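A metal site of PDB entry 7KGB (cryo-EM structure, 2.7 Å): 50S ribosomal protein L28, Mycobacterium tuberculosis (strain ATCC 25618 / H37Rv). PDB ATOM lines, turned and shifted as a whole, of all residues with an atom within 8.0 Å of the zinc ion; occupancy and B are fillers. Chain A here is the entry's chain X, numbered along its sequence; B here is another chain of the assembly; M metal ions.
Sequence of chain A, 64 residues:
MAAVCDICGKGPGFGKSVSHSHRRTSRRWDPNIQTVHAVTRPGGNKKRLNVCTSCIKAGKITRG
The backbone NH (N) of Lys 10 lies close to the side-chain sulfur (SG) of Cys 8 (3.7 Å). SG of Cys 5 sits close to N of Ile 7, 3.5 Å away. N of Cys 5 lies within hydrogen-bond range of O of Lys 10.
Within 4 Å of the zinc ion: Cys 5, Cys 8, Cys 52 and Cys 55. The nearest printed residue that does not touch the zinc ion is Ile 7 (4.5 Å).
The zinc ion is bound by SG of Cys 52 (2.3 Å), SG of Cys 55 (2.3 Å), SG of Cys 8 (2.3 Å) and SG of Cys 5 (2.3 Å). The zinc ion has four donor atoms within binding distance.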
ATOM      1  N   VAL A   4     -20.390  -9.463  13.639  1.00  0.00           N
ATOM      2  CA  VAL A   4     -19.302 -10.334  13.199  1.00  0.00           C
ATOM      3  C   VAL A   4     -19.869 -11.689  12.817  1.00  0.00           C
ATOM      4  O   VAL A   4     -20.633 -12.292  13.577  1.00  0.00           O
ATOM      5  CB  VAL A   4     -18.220 -10.498  14.282  1.00  0.00           C
ATOM      6  CG1 VAL A   4     -17.007 -11.166  13.700  1.00  0.00           C
ATOM      7  CG2 VAL A   4     -17.851  -9.139  14.848  1.00  0.00           C
ATOM      8  N   CYS A   5     -19.492 -12.175  11.633  1.00  0.00           N
ATOM      9  CA  CYS A   5     -19.934 -13.472  11.155  1.00  0.00           C
ATOM     10  C   CYS A   5     -19.074 -14.587  11.751  1.00  0.00           C
ATOM     11  O   CYS A   5     -17.851 -14.476  11.823  1.00  0.00           O
ATOM     12  CB  CYS A   5     -19.882 -13.526   9.631  1.00  0.00           C
ATOM     13  SG  CYS A   5     -20.391 -15.109   8.911  1.00  0.00           S
ATOM     14  N   ASP A   6     -19.726 -15.665  12.160  1.00  0.00           N
ATOM     15  CA  ASP A   6     -19.024 -16.760  12.822  1.00  0.00           C
ATOM     16  C   ASP A   6     -18.387 -17.742  11.858  1.00  0.00           C
ATOM     17  O   ASP A   6     -17.743 -18.685  12.304  1.00  0.00           O
ATOM     18  CB  ASP A   6     -19.981 -17.496  13.750  1.00  0.00           C
ATOM     19  CG  ASP A   6     -20.476 -16.637  14.884  1.00  0.00           C
ATOM     20  OD1 ASP A   6     -19.891 -15.544  15.082  1.00  0.00           O
ATOM     21  OD2 ASP A   6     -21.436 -17.034  15.568  1.00  0.00           O
ATOM     22  N   ILE A   7     -18.561 -17.558  10.554  1.00  0.00           N
ATOM     23  CA  ILE A   7     -17.955 -18.456   9.582  1.00  0.00           C
ATOM     24  C   ILE A   7     -16.772 -17.761   8.924  1.00  0.00           C
ATOM     25  O   ILE A   7     -15.623 -18.189   9.095  1.00  0.00           O
ATOM     26  CB  ILE A   7     -18.969 -18.901   8.527  1.00  0.00           C
ATOM     27  CG1 ILE A   7     -19.997 -19.834   9.138  1.00  0.00           C
ATOM     28  CG2 ILE A   7     -18.279 -19.593   7.377  1.00  0.00           C
ATOM     29  CD1 ILE A   7     -21.132 -20.133   8.219  1.00  0.00           C
ATOM     30  N   CYS A   8     -17.036 -16.691   8.191  1.00  0.00           N
ATOM     31  CA  CYS A   8     -16.010 -16.007   7.416  1.00  0.00           C
ATOM     32  C   CYS A   8     -15.407 -14.828   8.158  1.00  0.00           C
ATOM     33  O   CYS A   8     -14.514 -14.168   7.612  1.00  0.00           O
ATOM     34  CB  CYS A   8     -16.570 -15.537   6.076  1.00  0.00           C
ATOM     35  SG  CYS A   8     -17.937 -14.355   6.159  1.00  0.00           S
ATOM     36  N   GLY A   9     -15.861 -14.538   9.371  1.00  0.00           N
ATOM     37  CA  GLY A   9     -15.310 -13.439  10.136  1.00  0.00           C
ATOM     38  C   GLY A   9     -15.570 -12.065   9.565  1.00  0.00           C
ATOM     39  O   GLY A   9     -14.895 -11.121   9.953  1.00  0.00           O
ATOM     40  N   LYS A  10     -16.526 -11.941   8.651  1.00  0.00           N
ATOM     41  CA  LYS A  10     -16.831 -10.646   8.059  1.00  0.00           C
ATOM     42  C   LYS A  10     -17.323  -9.681   9.134  1.00  0.00           C
ATOM     43  O   LYS A  10     -18.310  -9.957   9.812  1.00  0.00           O
ATOM     44  CB  LYS A  10     -17.866 -10.818   6.955  1.00  0.00           C
ATOM     45  CG  LYS A  10     -18.648  -9.572   6.629  1.00  0.00           C
ATOM     46  CD  LYS A  10     -18.955  -9.490   5.151  1.00  0.00           C
ATOM     47  CE  LYS A  10     -20.026 -10.467   4.731  1.00  0.00           C
ATOM     48  NZ  LYS A  10     -20.166 -10.468   3.259  1.00  0.00           N
ATOM     49  N   GLY A  11     -16.632  -8.564   9.280  1.00  0.00           N
ATOM     50  CA  GLY A  11     -16.967  -7.605  10.293  1.00  0.00           C
ATOM     51  C   GLY A  11     -17.458  -6.306   9.702  1.00  0.00           C
ATOM     52  O   GLY A  11     -17.594  -6.173   8.482  1.00  0.00           O
ATOM     53  N   PRO A  31     -22.449  -5.914   8.568  1.00  0.00           N
ATOM     54  CA  PRO A  31     -22.893  -7.025   7.726  1.00  0.00           C
ATOM     55  C   PRO A  31     -24.265  -7.514   8.145  1.00  0.00           C
ATOM     56  O   PRO A  31     -24.675  -7.373   9.297  1.00  0.00           O
ATOM     57  CB  PRO A  31     -21.823  -8.085   7.941  1.00  0.00           C
ATOM     58  CG  PRO A  31     -21.207  -7.747   9.208  1.00  0.00           C
ATOM     59  CD  PRO A  31     -21.280  -6.276   9.383  1.00  0.00           C
ATOM     60  N   ASN A  32     -24.979  -8.101   7.193  1.00  0.00           N
ATOM     61  CA  ASN A  32     -26.331  -8.595   7.424  1.00  0.00           C
ATOM     62  C   ASN A  32     -26.228  -9.926   8.144  1.00  0.00           C
ATOM     63  O   ASN A  32     -26.216 -10.995   7.543  1.00  0.00           O
ATOM     64  CB  ASN A  32     -27.081  -8.735   6.112  1.00  0.00           C
ATOM     65  CG  ASN A  32     -28.561  -8.819   6.296  1.00  0.00           C
ATOM     66  OD1 ASN A  32     -29.055  -8.813   7.413  1.00  0.00           O
ATOM     67  ND2 ASN A  32     -29.289  -8.902   5.205  1.00  0.00           N
ATOM     68  N   ILE A  33     -26.171  -9.861   9.470  1.00  0.00           N
ATOM     69  CA  ILE A  33     -25.940 -11.044  10.298  1.00  0.00           C
ATOM     70  C   ILE A  33     -27.278 -11.564  10.786  1.00  0.00           C
ATOM     71  O   ILE A  33     -28.052 -10.818  11.387  1.00  0.00           O
ATOM     72  CB  ILE A  33     -25.011 -10.723  11.473  1.00  0.00           C
ATOM     73  CG1 ILE A  33     -23.690 -10.144  10.966  1.00  0.00           C
ATOM     74  CG2 ILE A  33     -24.776 -11.952  12.305  1.00  0.00           C
ATOM     75  CD1 ILE A  33     -22.811 -11.146  10.298  1.00  0.00           C
ATOM     76  N   ASN A  50     -24.253 -17.102  14.400  1.00  0.00           N
ATOM     77  CA  ASN A  50     -24.456 -15.761  13.862  1.00  0.00           C
ATOM     78  C   ASN A  50     -23.702 -15.686  12.548  1.00  0.00           C
ATOM     79  O   ASN A  50     -22.482 -15.501  12.540  1.00  0.00           O
ATOM     80  CB  ASN A  50     -23.960 -14.697  14.839  1.00  0.00           C
ATOM     81  CG  ASN A  50     -24.998 -14.333  15.864  1.00  0.00           C
ATOM     82  OD1 ASN A  50     -26.200 -14.443  15.627  1.00  0.00           O
ATOM     83  ND2 ASN A  50     -24.536 -13.889  17.022  1.00  0.00           N
ATOM     84  N   VAL A  51     -24.404 -15.831  11.440  1.00  0.00           N
ATOM     85  CA  VAL A  51     -23.765 -15.885  10.131  1.00  0.00           C
ATOM     86  C   VAL A  51     -24.385 -14.829   9.237  1.00  0.00           C
ATOM     87  O   VAL A  51     -25.487 -14.339   9.479  1.00  0.00           O
ATOM     88  CB  VAL A  51     -23.880 -17.281   9.498  1.00  0.00           C
ATOM     89  CG1 VAL A  51     -23.341 -18.317  10.445  1.00  0.00           C
ATOM     90  CG2 VAL A  51     -25.296 -17.575   9.177  1.00  0.00           C
ATOM     91  N   CYS A  52     -23.662 -14.470   8.191  1.00  0.00           N
ATOM     92  CA  CYS A  52     -24.131 -13.448   7.271  1.00  0.00           C
ATOM     93  C   CYS A  52     -24.965 -14.068   6.144  1.00  0.00           C
ATOM     94  O   CYS A  52     -24.892 -15.269   5.851  1.00  0.00           O
ATOM     95  CB  CYS A  52     -22.964 -12.659   6.682  1.00  0.00           C
ATOM     96  SG  CYS A  52     -21.744 -13.602   5.763  1.00  0.00           S
ATOM     97  N   THR A  53     -25.771 -13.216   5.531  1.00  0.00           N
ATOM     98  CA  THR A  53     -26.679 -13.695   4.499  1.00  0.00           C
ATOM     99  C   THR A  53     -25.929 -14.222   3.281  1.00  0.00           C
ATOM    100  O   THR A  53     -26.470 -15.036   2.541  1.00  0.00           O
ATOM    101  CB  THR A  53     -27.650 -12.601   4.086  1.00  0.00           C
ATOM    102  OG1 THR A  53     -26.925 -11.493   3.546  1.00  0.00           O
ATOM    103  CG2 THR A  53     -28.454 -12.152   5.264  1.00  0.00           C
ATOM    104  N   SER A  54     -24.681 -13.789   3.078  1.00  0.00           N
ATOM    105  CA  SER A  54     -23.891 -14.382   2.001  1.00  0.00           C
ATOM    106  C   SER A  54     -23.558 -15.843   2.292  1.00  0.00           C
ATOM    107  O   SER A  54     -23.691 -16.694   1.406  1.00  0.00           O
ATOM    108  CB  SER A  54     -22.603 -13.580   1.806  1.00  0.00           C
ATOM    109  OG  SER A  54     -22.904 -12.266   1.370  1.00  0.00           O
ATOM    110  N   CYS A  55     -23.165 -16.155   3.524  1.00  0.00           N
ATOM    111  CA  CYS A  55     -22.944 -17.545   3.890  1.00  0.00           C
ATOM    112  C   CYS A  55     -24.233 -18.354   3.858  1.00  0.00           C
ATOM    113  O   CYS A  55     -24.217 -19.525   3.478  1.00  0.00           O
ATOM    114  CB  CYS A  55     -22.310 -17.643   5.277  1.00  0.00           C
ATOM    115  SG  CYS A  55     -20.641 -16.969   5.423  1.00  0.00           S
ATOM    116  N   ILE A  56     -25.356 -17.754   4.250  1.00  0.00           N
ATOM    117  CA  ILE A  56     -26.622 -18.458   4.144  1.00  0.00           C
ATOM    118  C   ILE A  56     -26.971 -18.722   2.677  1.00  0.00           C
ATOM    119  O   ILE A  56     -27.441 -19.803   2.324  1.00  0.00           O
ATOM    120  CB  ILE A  56     -27.738 -17.672   4.849  1.00  0.00           C
ATOM    121  CG1 ILE A  56     -27.367 -17.440   6.302  1.00  0.00           C
ATOM    122  CG2 ILE A  56     -29.045 -18.428   4.775  1.00  0.00           C
ATOM    123  CD1 ILE A  56     -28.350 -16.577   7.045  1.00  0.00           C
ATOM    124  N   LYS A  60     -22.947 -22.850   2.802  1.00  0.00           N
ATOM    125  CA  LYS A  60     -21.945 -22.975   3.849  1.00  0.00           C
ATOM    126  C   LYS A  60     -22.460 -23.771   5.047  1.00  0.00           C
ATOM    127  O   LYS A  60     -21.729 -24.596   5.597  1.00  0.00           O
ATOM    128  CB  LYS A  60     -21.458 -21.602   4.293  1.00  0.00           C
ATOM    129  CG  LYS A  60     -20.686 -20.859   3.216  1.00  0.00           C
ATOM    130  CD  LYS A  60     -19.366 -21.551   2.940  1.00  0.00           C
ATOM    131  CE  LYS A  60     -18.497 -20.746   1.998  1.00  0.00           C
ATOM    132  NZ  LYS A  60     -19.008 -20.743   0.600  1.00  0.00           N
ATOM    133  P     U B 486     -22.708  -7.528   3.879  1.00  0.00           P
ATOM    134  OP1   U B 486     -23.324  -8.444   4.858  1.00  0.00           O
ATOM    135  OP2   U B 486     -21.807  -8.049   2.832  1.00  0.00           O
ATOM    136  O5'   U B 486     -23.874  -6.737   3.153  1.00  0.00           O
ATOM    137  C5'   U B 486     -24.956  -6.176   3.880  1.00  0.00           C
ATOM    138  C4'   U B 486     -25.978  -5.569   2.956  1.00  0.00           C
ATOM    139  O4'   U B 486     -25.403  -4.434   2.278  1.00  0.00           O
ATOM    140  C3'   U B 486     -26.462  -6.462   1.823  1.00  0.00           C
ATOM    141  O3'   U B 486     -27.454  -7.380   2.218  1.00  0.00           O
ATOM    142  C2'   U B 486     -26.949  -5.456   0.803  1.00  0.00           C
ATOM    143  O2'   U B 486     -28.220  -4.966   1.181  1.00  0.00           O
ATOM    144  C1'   U B 486     -25.941  -4.330   0.975  1.00  0.00           C
ATOM    145  N1    U B 486     -24.835  -4.386   0.006  1.00  0.00           N
ATOM    146  C2    U B 486     -25.068  -3.937  -1.267  1.00  0.00           C
ATOM    147  O2    U B 486     -26.147  -3.519  -1.625  1.00  0.00           O
ATOM    148  N3    U B 486     -24.008  -4.016  -2.118  1.00  0.00           N
ATOM    149  C4    U B 486     -22.753  -4.473  -1.814  1.00  0.00           C
ATOM    150  O4    U B 486     -21.888  -4.484  -2.672  1.00  0.00           O
ATOM    151  C5    U B 486     -22.583  -4.919  -0.475  1.00  0.00           C
ATOM    152  C6    U B 486     -23.612  -4.867   0.372  1.00  0.00           C
HETATM  153 ZN    ZN M   1     -20.117 -15.034   6.601  1.00  0.00          ZN
